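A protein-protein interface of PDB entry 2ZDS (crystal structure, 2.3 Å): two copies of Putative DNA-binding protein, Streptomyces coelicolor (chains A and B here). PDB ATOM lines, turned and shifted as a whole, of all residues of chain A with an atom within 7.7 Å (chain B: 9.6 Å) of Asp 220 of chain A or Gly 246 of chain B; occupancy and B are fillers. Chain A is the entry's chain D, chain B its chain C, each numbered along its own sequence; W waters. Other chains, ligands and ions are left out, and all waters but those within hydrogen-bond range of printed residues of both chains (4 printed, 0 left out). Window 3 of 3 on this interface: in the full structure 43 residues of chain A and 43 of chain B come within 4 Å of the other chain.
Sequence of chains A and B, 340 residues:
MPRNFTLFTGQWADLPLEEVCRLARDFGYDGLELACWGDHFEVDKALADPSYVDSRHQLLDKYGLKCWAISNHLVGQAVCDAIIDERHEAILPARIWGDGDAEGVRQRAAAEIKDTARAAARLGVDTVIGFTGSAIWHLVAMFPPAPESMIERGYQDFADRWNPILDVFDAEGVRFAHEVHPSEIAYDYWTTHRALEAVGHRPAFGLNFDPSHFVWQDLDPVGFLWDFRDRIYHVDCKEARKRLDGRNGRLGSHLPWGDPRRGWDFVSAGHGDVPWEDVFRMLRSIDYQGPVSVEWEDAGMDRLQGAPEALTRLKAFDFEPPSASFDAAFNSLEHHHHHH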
ATOM      1  N   TYR A 189      24.814 -10.100  26.523  1.00  0.00           N
ATOM      2  CA  TYR A 189      24.530  -9.252  25.387  1.00  0.00           C
ATOM      3  C   TYR A 189      22.990  -9.136  25.116  1.00  0.00           C
ATOM      4  O   TYR A 189      22.447  -8.035  25.111  1.00  0.00           O
ATOM      5  CB  TYR A 189      25.315  -9.732  24.126  1.00  0.00           C
ATOM      6  CG  TYR A 189      25.043  -8.872  22.931  1.00  0.00           C
ATOM      7  CD1 TYR A 189      23.908  -9.076  22.147  1.00  0.00           C
ATOM      8  CD2 TYR A 189      25.906  -7.821  22.589  1.00  0.00           C
ATOM      9  CE1 TYR A 189      23.635  -8.238  21.036  1.00  0.00           C
ATOM     10  CE2 TYR A 189      25.640  -6.986  21.494  1.00  0.00           C
ATOM     11  CZ  TYR A 189      24.515  -7.213  20.718  1.00  0.00           C
ATOM     12  OH  TYR A 189      24.259  -6.387  19.642  1.00  0.00           O
ATOM     13  N   TRP A 190      22.306 -10.272  24.908  1.00  0.00           N
ATOM     14  CA  TRP A 190      20.900 -10.247  24.513  1.00  0.00           C
ATOM     15  C   TRP A 190      19.978  -9.820  25.631  1.00  0.00           C
ATOM     16  O   TRP A 190      18.939  -9.194  25.348  1.00  0.00           O
ATOM     17  CB  TRP A 190      20.428 -11.594  23.911  1.00  0.00           C
ATOM     18  CG  TRP A 190      21.076 -11.870  22.589  1.00  0.00           C
ATOM     19  CD1 TRP A 190      21.944 -12.888  22.290  1.00  0.00           C
ATOM     20  CD2 TRP A 190      20.953 -11.070  21.380  1.00  0.00           C
ATOM     21  NE1 TRP A 190      22.387 -12.764  20.986  1.00  0.00           N
ATOM     22  CE2 TRP A 190      21.798 -11.670  20.399  1.00  0.00           C
ATOM     23  CE3 TRP A 190      20.216  -9.913  21.041  1.00  0.00           C
ATOM     24  CZ2 TRP A 190      21.919 -11.162  19.087  1.00  0.00           C
ATOM     25  CZ3 TRP A 190      20.338  -9.390  19.721  1.00  0.00           C
ATOM     26  CH2 TRP A 190      21.189 -10.029  18.762  1.00  0.00           C
ATOM     27  N   PHE A 209      30.517  -1.139  32.498  1.00  0.00           N
ATOM     28  CA  PHE A 209      31.173  -2.161  31.716  1.00  0.00           C
ATOM     29  C   PHE A 209      32.264  -2.863  32.534  1.00  0.00           C
ATOM     30  O   PHE A 209      33.205  -2.235  33.008  1.00  0.00           O
ATOM     31  CB  PHE A 209      31.792  -1.543  30.495  1.00  0.00           C
ATOM     32  CG  PHE A 209      32.636  -2.495  29.709  1.00  0.00           C
ATOM     33  CD1 PHE A 209      32.043  -3.578  29.019  1.00  0.00           C
ATOM     34  CD2 PHE A 209      34.020  -2.330  29.660  1.00  0.00           C
ATOM     35  CE1 PHE A 209      32.834  -4.459  28.271  1.00  0.00           C
ATOM     36  CE2 PHE A 209      34.816  -3.198  28.889  1.00  0.00           C
ATOM     37  CZ  PHE A 209      34.221  -4.256  28.211  1.00  0.00           C
ATOM     38  N   PHE A 214      32.263 -11.554  30.798  1.00  0.00           N
ATOM     39  CA  PHE A 214      32.220 -11.804  29.328  1.00  0.00           C
ATOM     40  C   PHE A 214      33.093 -13.001  28.960  1.00  0.00           C
ATOM     41  O   PHE A 214      32.737 -13.734  28.066  1.00  0.00           O
ATOM     42  CB  PHE A 214      32.634 -10.572  28.537  1.00  0.00           C
ATOM     43  CG  PHE A 214      31.621  -9.455  28.596  1.00  0.00           C
ATOM     44  CD1 PHE A 214      31.278  -8.845  29.824  1.00  0.00           C
ATOM     45  CD2 PHE A 214      31.009  -8.998  27.429  1.00  0.00           C
ATOM     46  CE1 PHE A 214      30.328  -7.795  29.874  1.00  0.00           C
ATOM     47  CE2 PHE A 214      30.096  -7.950  27.470  1.00  0.00           C
ATOM     48  CZ  PHE A 214      29.751  -7.342  28.678  1.00  0.00           C
ATOM     49  N   VAL A 215      34.163 -13.236  29.737  1.00  0.00           N
ATOM     50  CA  VAL A 215      35.083 -14.378  29.527  1.00  0.00           C
ATOM     51  C   VAL A 215      34.460 -15.768  29.627  1.00  0.00           C
ATOM     52  O   VAL A 215      34.465 -16.522  28.637  1.00  0.00           O
ATOM     53  CB  VAL A 215      36.376 -14.268  30.401  1.00  0.00           C
ATOM     54  CG1 VAL A 215      37.297 -15.469  30.193  1.00  0.00           C
ATOM     55  CG2 VAL A 215      37.116 -12.914  30.128  1.00  0.00           C
ATOM     56  N   GLN A 217      31.354 -16.649  29.658  1.00  0.00           N
ATOM     57  CA  GLN A 217      30.159 -16.664  28.809  1.00  0.00           C
ATOM     58  C   GLN A 217      30.419 -16.599  27.282  1.00  0.00           C
ATOM     59  O   GLN A 217      29.448 -16.691  26.491  1.00  0.00           O
ATOM     60  CB  GLN A 217      29.251 -15.490  29.201  1.00  0.00           C
ATOM     61  CG  GLN A 217      28.499 -15.690  30.478  1.00  0.00           C
ATOM     62  CD  GLN A 217      27.488 -14.560  30.726  1.00  0.00           C
ATOM     63  OE1 GLN A 217      27.829 -13.474  31.227  1.00  0.00           O
ATOM     64  NE2 GLN A 217      26.247 -14.807  30.356  1.00  0.00           N
ATOM     65  N   ASP A 218      31.697 -16.423  26.896  1.00  0.00           N
ATOM     66  CA  ASP A 218      32.158 -16.303  25.510  1.00  0.00           C
ATOM     67  C   ASP A 218      31.546 -15.117  24.756  1.00  0.00           C
ATOM     68  O   ASP A 218      31.294 -15.177  23.532  1.00  0.00           O
ATOM     69  CB  ASP A 218      31.929 -17.613  24.730  1.00  0.00           C
ATOM     70  CG  ASP A 218      33.048 -18.605  24.889  1.00  0.00           C
ATOM     71  OD1 ASP A 218      34.121 -18.275  25.433  1.00  0.00           O
ATOM     72  OD2 ASP A 218      32.856 -19.770  24.523  1.00  0.00           O
ATOM     73  N   LEU A 219      31.308 -14.032  25.494  1.00  0.00           N
ATOM     74  CA  LEU A 219      30.763 -12.834  24.924  1.00  0.00           C
ATOM     75  C   LEU A 219      31.954 -11.973  24.476  1.00  0.00           C
ATOM     76  O   LEU A 219      32.993 -11.890  25.176  1.00  0.00           O
ATOM     77  CB  LEU A 219      29.935 -12.102  25.993  1.00  0.00           C
ATOM     78  CG  LEU A 219      28.720 -12.821  26.608  1.00  0.00           C
ATOM     79  CD1 LEU A 219      28.227 -11.990  27.785  1.00  0.00           C
ATOM     80  CD2 LEU A 219      27.642 -13.034  25.549  1.00  0.00           C
ATOM     81  N   ASP A 220      31.825 -11.370  23.302  1.00  0.00           N
ATOM     82  CA  ASP A 220      32.788 -10.391  22.803  1.00  0.00           C
ATOM     83  C   ASP A 220      32.580  -9.032  23.546  1.00  0.00           C
ATOM     84  O   ASP A 220      31.593  -8.369  23.317  1.00  0.00           O
ATOM     85  CB  ASP A 220      32.603 -10.270  21.279  1.00  0.00           C
ATOM     86  CG  ASP A 220      33.591  -9.299  20.594  1.00  0.00           C
ATOM     87  OD1 ASP A 220      34.419  -8.663  21.244  1.00  0.00           O
ATOM     88  OD2 ASP A 220      33.526  -9.177  19.365  1.00  0.00           O
ATOM     89  N   PRO A 221      33.512  -8.644  24.457  1.00  0.00           N
ATOM     90  CA  PRO A 221      33.364  -7.351  25.206  1.00  0.00           C
ATOM     91  C   PRO A 221      33.449  -6.087  24.331  1.00  0.00           C
ATOM     92  O   PRO A 221      32.832  -5.065  24.654  1.00  0.00           O
ATOM     93  CB  PRO A 221      34.543  -7.370  26.197  1.00  0.00           C
ATOM     94  CG  PRO A 221      35.560  -8.350  25.545  1.00  0.00           C
ATOM     95  CD  PRO A 221      34.727  -9.398  24.877  1.00  0.00           C
ATOM     96  N   VAL A 222      34.198  -6.205  23.227  1.00  0.00           N
ATOM     97  CA  VAL A 222      34.493  -5.129  22.290  1.00  0.00           C
ATOM     98  C   VAL A 222      33.275  -4.816  21.424  1.00  0.00           C
ATOM     99  O   VAL A 222      32.919  -3.668  21.276  1.00  0.00           O
ATOM    100  CB  VAL A 222      35.815  -5.442  21.457  1.00  0.00           C
ATOM    101  CG1 VAL A 222      36.068  -4.416  20.407  1.00  0.00           C
ATOM    102  CG2 VAL A 222      37.036  -5.540  22.373  1.00  0.00           C
ATOM    103  N   GLY A 223      32.589  -5.812  20.883  1.00  0.00           N
ATOM    104  CA  GLY A 223      31.290  -5.579  20.171  1.00  0.00           C
ATOM    105  C   GLY A 223      30.170  -5.058  21.040  1.00  0.00           C
ATOM    106  O   GLY A 223      29.270  -4.335  20.582  1.00  0.00           O
ATOM    107  N   PHE A 224      30.183  -5.470  22.307  1.00  0.00           N
ATOM    108  CA  PHE A 224      29.232  -5.013  23.300  1.00  0.00           C
ATOM    109  C   PHE A 224      29.419  -3.519  23.456  1.00  0.00           C
ATOM    110  O   PHE A 224      28.447  -2.741  23.401  1.00  0.00           O
ATOM    111  CB  PHE A 224      29.495  -5.739  24.638  1.00  0.00           C
ATOM    112  CG  PHE A 224      28.562  -5.362  25.744  1.00  0.00           C
ATOM    113  CD1 PHE A 224      28.814  -4.212  26.550  1.00  0.00           C
ATOM    114  CD2 PHE A 224      27.441  -6.168  26.043  1.00  0.00           C
ATOM    115  CE1 PHE A 224      27.950  -3.877  27.645  1.00  0.00           C
ATOM    116  CE2 PHE A 224      26.550  -5.829  27.130  1.00  0.00           C
ATOM    117  CZ  PHE A 224      26.792  -4.703  27.925  1.00  0.00           C
ATOM    118  N   LEU A 225      30.678  -3.130  23.664  1.00  0.00           N
ATOM    119  CA  LEU A 225      31.067  -1.707  23.806  1.00  0.00           C
ATOM    120  C   LEU A 225      30.581  -0.891  22.615  1.00  0.00           C
ATOM    121  O   LEU A 225      30.060   0.190  22.799  1.00  0.00           O
ATOM    122  CB  LEU A 225      32.590  -1.557  23.957  1.00  0.00           C
ATOM    123  CG  LEU A 225      33.138  -1.828  25.361  1.00  0.00           C
ATOM    124  CD1 LEU A 225      34.684  -1.893  25.397  1.00  0.00           C
ATOM    125  CD2 LEU A 225      32.615  -0.792  26.431  1.00  0.00           C
ATOM    126  N   TRP A 226      30.720  -1.441  21.410  1.00  0.00           N
ATOM    127  CA  TRP A 226      30.273  -0.785  20.185  1.00  0.00           C
ATOM    128  C   TRP A 226      28.750  -0.672  20.090  1.00  0.00           C
ATOM    129  O   TRP A 226      28.220   0.428  19.866  1.00  0.00           O
ATOM    130  CB  TRP A 226      30.794  -1.545  18.979  1.00  0.00           C
ATOM    131  CG  TRP A 226      30.376  -0.978  17.680  1.00  0.00           C
ATOM    132  CD1 TRP A 226      29.396  -1.454  16.855  1.00  0.00           C
ATOM    133  CD2 TRP A 226      30.925   0.172  17.026  1.00  0.00           C
ATOM    134  NE1 TRP A 226      29.299  -0.667  15.732  1.00  0.00           N
ATOM    135  CE2 TRP A 226      30.239   0.326  15.804  1.00  0.00           C
ATOM    136  CE3 TRP A 226      31.928   1.096  17.362  1.00  0.00           C
ATOM    137  CZ2 TRP A 226      30.528   1.369  14.893  1.00  0.00           C
ATOM    138  CZ3 TRP A 226      32.227   2.131  16.453  1.00  0.00           C
ATOM    139  CH2 TRP A 226      31.527   2.250  15.225  1.00  0.00           C
ATOM    140  N   PRO A 275      40.610  -9.282  26.696  1.00  0.00           N
ATOM    141  CA  PRO A 275      41.421  -8.655  25.628  1.00  0.00           C
ATOM    142  C   PRO A 275      41.598  -7.131  25.801  1.00  0.00           C
ATOM    143  O   PRO A 275      40.983  -6.347  25.097  1.00  0.00           O
ATOM    144  CB  PRO A 275      40.629  -9.013  24.335  1.00  0.00           C
ATOM    145  CG  PRO A 275      39.168  -9.200  24.814  1.00  0.00           C
ATOM    146  CD  PRO A 275      39.228  -9.612  26.245  1.00  0.00           C
ATOM    147  N   ASP A 278      42.171  -4.587  22.722  1.00  0.00           N
ATOM    148  CA  ASP A 278      40.946  -4.220  22.028  1.00  0.00           C
ATOM    149  C   ASP A 278      39.972  -3.381  22.848  1.00  0.00           C
ATOM    150  O   ASP A 278      39.415  -2.399  22.332  1.00  0.00           O
ATOM    151  CB  ASP A 278      40.290  -5.447  21.423  1.00  0.00           C
ATOM    152  CG  ASP A 278      41.166  -6.085  20.379  1.00  0.00           C
ATOM    153  OD1 ASP A 278      41.751  -5.347  19.548  1.00  0.00           O
ATOM    154  OD2 ASP A 278      41.278  -7.317  20.400  1.00  0.00           O
ATOM    155  N   VAL A 279      39.785  -3.749  24.114  1.00  0.00           N
ATOM    156  CA  VAL A 279      38.914  -2.976  25.006  1.00  0.00           C
ATOM    157  C   VAL A 279      39.348  -1.512  25.040  1.00  0.00           C
ATOM    158  O   VAL A 279      38.550  -0.624  24.783  1.00  0.00           O
ATOM    159  CB  VAL A 279      38.824  -3.609  26.439  1.00  0.00           C
ATOM    160  CG1 VAL A 279      38.218  -2.634  27.496  1.00  0.00           C
ATOM    161  CG2 VAL A 279      38.069  -4.994  26.405  1.00  0.00           C
ATOM    162  N   MET A 282      38.794   0.312  21.859  1.00  0.00           N
ATOM    163  CA  MET A 282      37.384   0.533  21.630  1.00  0.00           C
ATOM    164  C   MET A 282      36.812   1.646  22.515  1.00  0.00           C
ATOM    165  O   MET A 282      35.962   2.379  22.079  1.00  0.00           O
ATOM    166  CB  MET A 282      36.592  -0.780  21.742  1.00  0.00           C
ATOM    167  CG  MET A 282      35.114  -0.601  21.542  1.00  0.00           C
ATOM    168  SD  MET A 282      34.676   0.022  19.701  1.00  0.00           S
ATOM    169  CE  MET A 282      34.754  -1.635  18.638  1.00  0.00           C
ATOM    170  N   ARG B 243      26.526 -22.069  18.869  1.00  0.00           N
ATOM    171  CA  ARG B 243      26.702 -21.011  17.892  1.00  0.00           C
ATOM    172  C   ARG B 243      27.050 -19.719  18.635  1.00  0.00           C
ATOM    173  O   ARG B 243      26.237 -18.822  18.809  1.00  0.00           O
ATOM    174  CB  ARG B 243      25.460 -20.839  17.005  1.00  0.00           C
ATOM    175  CG  ARG B 243      25.785 -20.256  15.680  1.00  0.00           C
ATOM    176  CD  ARG B 243      24.516 -19.719  15.026  1.00  0.00           C
ATOM    177  NE  ARG B 243      24.984 -18.424  14.661  1.00  0.00           N
ATOM    178  CZ  ARG B 243      24.350 -17.281  14.746  1.00  0.00           C
ATOM    179  NH1 ARG B 243      25.018 -16.224  14.344  1.00  0.00           N
ATOM    180  NH2 ARG B 243      23.111 -17.189  15.164  1.00  0.00           N
ATOM    181  N   LEU B 244      28.299 -19.643  19.020  1.00  0.00           N
ATOM    182  CA  LEU B 244      28.809 -18.565  19.855  1.00  0.00           C
ATOM    183  C   LEU B 244      29.495 -17.554  18.951  1.00  0.00           C
ATOM    184  O   LEU B 244      30.670 -17.693  18.662  1.00  0.00           O
ATOM    185  CB  LEU B 244      29.840 -19.137  20.835  1.00  0.00           C
ATOM    186  CG  LEU B 244      29.578 -19.780  22.219  1.00  0.00           C
ATOM    187  CD1 LEU B 244      28.215 -19.467  22.783  1.00  0.00           C
ATOM    188  CD2 LEU B 244      29.939 -21.267  22.352  1.00  0.00           C
ATOM    189  N   ASP B 245      28.754 -16.561  18.487  1.00  0.00           N
ATOM    190  CA  ASP B 245      29.254 -15.568  17.506  1.00  0.00           C
ATOM    191  C   ASP B 245      29.754 -14.232  18.118  1.00  0.00           C
ATOM    192  O   ASP B 245      29.841 -13.227  17.385  1.00  0.00           O
ATOM    193  CB  ASP B 245      28.123 -15.266  16.493  1.00  0.00           C
ATOM    194  CG  ASP B 245      26.912 -14.558  17.133  1.00  0.00           C
ATOM    195  OD1 ASP B 245      26.844 -14.420  18.396  1.00  0.00           O
ATOM    196  OD2 ASP B 245      25.999 -14.108  16.368  1.00  0.00           O
ATOM    197  N   GLY B 246      30.051 -14.188  19.434  1.00  0.00           N
ATOM    198  CA  GLY B 246      30.361 -12.912  20.107  1.00  0.00           C
ATOM    199  C   GLY B 246      29.173 -12.242  20.808  1.00  0.00           C
ATOM    200  O   GLY B 246      29.326 -11.583  21.866  1.00  0.00           O
ATOM    201  N   ARG B 247      27.973 -12.432  20.249  1.00  0.00           N
ATOM    202  CA  ARG B 247      26.730 -11.873  20.843  1.00  0.00           C
ATOM    203  C   ARG B 247      25.992 -12.909  21.649  1.00  0.00           C
ATOM    204  O   ARG B 247      25.536 -12.631  22.766  1.00  0.00           O
ATOM    205  CB  ARG B 247      25.762 -11.337  19.780  1.00  0.00           C
ATOM    206  CG  ARG B 247      26.173 -10.053  19.107  1.00  0.00           C
ATOM    207  CD  ARG B 247      25.665  -9.917  17.668  1.00  0.00           C
ATOM    208  NE  ARG B 247      26.745  -9.288  16.883  1.00  0.00           N
ATOM    209  CZ  ARG B 247      27.686  -9.935  16.155  1.00  0.00           C
ATOM    210  NH1 ARG B 247      28.652  -9.241  15.509  1.00  0.00           N
ATOM    211  NH2 ARG B 247      27.655 -11.261  16.029  1.00  0.00           N
ATOM    212  N   ASN B 248      25.794 -14.074  21.050  1.00  0.00           N
ATOM    213  CA  ASN B 248      25.108 -15.180  21.709  1.00  0.00           C
ATOM    214  C   ASN B 248      25.979 -15.615  22.908  1.00  0.00           C
ATOM    215  O   ASN B 248      27.206 -15.619  22.792  1.00  0.00           O
ATOM    216  CB  ASN B 248      24.949 -16.368  20.751  1.00  0.00           C
ATOM    217  CG  ASN B 248      24.103 -16.059  19.540  1.00  0.00           C
ATOM    218  OD1 ASN B 248      23.521 -14.963  19.409  1.00  0.00           O
ATOM    219  ND2 ASN B 248      23.991 -17.046  18.645  1.00  0.00           N
ATOM    220  N   GLY B 249      25.376 -15.961  24.041  1.00  0.00           N
ATOM    221  CA  GLY B 249      26.181 -16.409  25.172  1.00  0.00           C
ATOM    222  C   GLY B 249      25.979 -17.870  25.592  1.00  0.00           C
ATOM    223  O   GLY B 249      25.004 -18.502  25.236  1.00  0.00           O
ATOM    224  N   ARG B 250      26.907 -18.398  26.375  1.00  0.00           N
ATOM    225  CA  ARG B 250      26.851 -19.780  26.847  1.00  0.00           C
ATOM    226  C   ARG B 250      25.609 -20.185  27.646  1.00  0.00           C
ATOM    227  O   ARG B 250      25.284 -21.383  27.702  1.00  0.00           O
ATOM    228  CB  ARG B 250      28.109 -20.069  27.668  1.00  0.00           C
ATOM    229  CG  ARG B 250      29.368 -20.044  26.805  1.00  0.00           C
ATOM    230  CD  ARG B 250      29.960 -21.382  26.712  1.00  0.00           C
ATOM    231  NE  ARG B 250      31.052 -21.451  25.774  1.00  0.00           N
ATOM    232  CZ  ARG B 250      31.565 -22.601  25.358  1.00  0.00           C
ATOM    233  NH1 ARG B 250      31.070 -23.728  25.853  1.00  0.00           N
ATOM    234  NH2 ARG B 250      32.527 -22.633  24.434  1.00  0.00           N
ATOM    235  N   SER B 253      20.586 -16.858  27.383  1.00  0.00           N
ATOM    236  CA  SER B 253      19.872 -15.579  27.514  1.00  0.00           C
ATOM    237  C   SER B 253      18.376 -15.697  27.909  1.00  0.00           C
ATOM    238  O   SER B 253      17.597 -14.794  27.624  1.00  0.00           O
ATOM    239  CB  SER B 253      20.084 -14.660  26.287  1.00  0.00           C
ATOM    240  OG  SER B 253      21.431 -14.718  25.857  1.00  0.00           O
ATOM    241  N   ARG B 261      19.486 -16.644  18.680  1.00  0.00           N
ATOM    242  CA  ARG B 261      20.333 -15.834  19.561  1.00  0.00           C
ATOM    243  C   ARG B 261      20.869 -16.595  20.794  1.00  0.00           C
ATOM    244  O   ARG B 261      21.617 -16.033  21.600  1.00  0.00           O
ATOM    245  CB  ARG B 261      19.619 -14.529  19.933  1.00  0.00           C
ATOM    246  CG  ARG B 261      19.253 -13.704  18.646  1.00  0.00           C
ATOM    247  CD  ARG B 261      18.253 -12.592  18.981  1.00  0.00           C
ATOM    248  NE  ARG B 261      17.005 -13.143  19.473  1.00  0.00           N
ATOM    249  CZ  ARG B 261      16.103 -12.452  20.173  1.00  0.00           C
ATOM    250  NH1 ARG B 261      16.355 -11.192  20.477  1.00  0.00           N
ATOM    251  NH2 ARG B 261      14.961 -13.027  20.603  1.00  0.00           N
ATOM    252  N   ARG B 262      20.477 -17.864  20.936  1.00  0.00           N
ATOM    253  CA  ARG B 262      21.007 -18.763  21.953  1.00  0.00           C
ATOM    254  C   ARG B 262      22.448 -19.150  21.604  1.00  0.00           C
ATOM    255  O   ARG B 262      22.701 -19.497  20.442  1.00  0.00           O
ATOM    256  CB  ARG B 262      20.225 -20.064  21.914  1.00  0.00           C
ATOM    257  CG  ARG B 262      18.773 -20.086  22.470  1.00  0.00           C
ATOM    258  CD  ARG B 262      18.494 -21.582  22.844  1.00  0.00           C
ATOM    259  NE  ARG B 262      18.031 -21.422  24.170  1.00  0.00           N
ATOM    260  CZ  ARG B 262      18.657 -21.703  25.290  1.00  0.00           C
ATOM    261  NH1 ARG B 262      19.762 -22.410  25.321  1.00  0.00           N
ATOM    262  NH2 ARG B 262      18.063 -21.287  26.405  1.00  0.00           N
ATOM    263  N   GLY B 263      23.379 -19.130  22.568  1.00  0.00           N
ATOM    264  CA  GLY B 263      24.780 -19.606  22.309  1.00  0.00           C
ATOM    265  C   GLY B 263      24.859 -21.096  22.002  1.00  0.00           C
ATOM    266  O   GLY B 263      25.850 -21.579  21.465  1.00  0.00           O
HETATM  267  O   HOH W   1      25.315 -16.005  28.265  1.00  0.00           O
HETATM  268  O   HOH W   2      29.564 -15.914  21.560  1.00  0.00           O
HETATM  269  O   HOH W   3      29.034  -8.975  22.884  1.00  0.00           O
HETATM  270  O   HOH W   4      24.115 -12.669  24.973  1.00  0.00           O
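Among the printed residues, merely in contact across the chains: Tyr 189 of chain A with Arg 247 of chain B, Leu 219 of chain A with Arg 247 of chain B, Gln 217 of chain A with Gly 249 of chain B, Leu 219 of chain A with Gly 246 of chain B, Trp 190 of chain A with Arg 247 of chain B, Leu 219 of chain A with Gly 249 of chain B, Leu 219 of chain A with Asn 248 of chain B, Trp 190 of chain A with Ser 253 of chain B and Asp 218 of chain A with Leu 244 of chain B.
No position is printed for both chains.
Of the 14 pairs that touch across the chains among the printed residues, none has its exchanged pair printed and touching as well.
The side-chain amide oxygen (OD1) of Asn 248 of chain B is in hydrogen-bond range of the indole nitrogen (NE1) of Trp 190 of chain A (2.9 Å).
The side-chain carboxylate of Asp 218 of chain A lies within salt-bridge range of the guanidinium group of Arg 250 of chain B (2.8 Å).
The backbone NH (N) of Arg 250 of chain B is in hydrogen-bond range of the backbone carbonyl oxygen (O) of Gln 217 of chain A.
O of Gly 246 of chain B is in hydrogen-bond range of N of Asp 220 of chain A, 2.9 Å away.
The indole nitrogen (NE1) of Trp 190 of chain A lies close to the backbone carbonyl oxygen (O) of Arg 261 of chain B (3.4 Å).
Of the printed residues of chain B, Tyr 189 of chain A touches Arg 247.
Of the printed residues of chain B, Leu 219 of chain A touches Gly 246, Arg 247, Asn 248 and Gly 249.
Val 222 of chain A touches none of the printed residues of chain B.
No residue of chain B comes within 4 Å of Gly 223 of chain A.
Gly 246 of chain B touches just these residues of chain A: Leu 219 (3.6 Å) and Asp 220 (2.9 Å).
Of the printed residues of chain A, Arg 247 of chain B touches Tyr 189, Trp 190 and Leu 219.
Printed residues of chain A within 4 Å of Arg 250 of chain B: Gln 217 (3.1 Å) and Asp 218 (2.8 Å).
The nearest residue of chain B that does not touch Asp 220 of chain A is Arg 247 of chain B (5.0 Å).
The nearest printed residue of chain A that does not touch Leu 244 of chain B is Gln 217 of chain A (4.8 Å).
Hydrophobic or aromatic side chains of chain A that line the printed part of chain B: Tyr 189, Trp 190 and Leu 219.
Of the 12 printed residues of chain B, 8 touch a printed residue of chain A.
Among the printed residues, Asp or Glu carboxylates within 4 Å of a Lys or Arg side-chain nitrogen of the other chain: Asp 218 of chain A with Arg 250 of chain B (2.8 Å).
The backbone carbonyl oxygen (O) of Phe 214 of chain A lies within hydrogen-bond range of the backbone NH (N) of Leu 219 of chain A (3.0 Å).
O of Arg 261 of chain B sits close to OD1 of Asn 248 of chain B (3.1 Å).
The side-chain carboxylate of Asp 245 of chain B is in hydrogen-bond range of the backbone NH of Asn 248 of chain B.
The side-chain amide nitrogen of Asn 248 of chain B lies within hydrogen-bond range of the backbone carbonyl oxygen of Arg 262 of chain B, 3.3 Å away.
The backbone NH (N) of Gly 223 of chain A is in hydrogen-bond range of the side-chain carboxylate (OD1) of Asp 220 of chain A (3.4 Å).
The backbone carbonyl oxygen (O) of Arg 243 of chain B sits at hydrogen-bond distance from the side-chain amide nitrogen (ND2) of Asn 248 of chain B (2.9 Å).
Water W1 lies within hydrogen-bond range of NE2 of Gln 217 of chain A and N of Arg 250 of chain B.
Water W4 lies within hydrogen-bond range of O of Arg 247 of chain B (2.6 Å), N of Trp 190 of chain A (3.0 Å), N of Tyr 189 of chain A (3.1 Å) and OG of Ser 253 of chain B (3.5 Å).
Water W3 lies within hydrogen-bond range of O of Asp 220 of chain A (2.7 Å) and O of Gly 246 of chain B (2.8 Å).
Water W2 lies within hydrogen-bond range of O of Asn 248 of chain B, O of Asp 218 of chain A, N of Gly 246 of chain B and N of Asp 245 of chain B.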
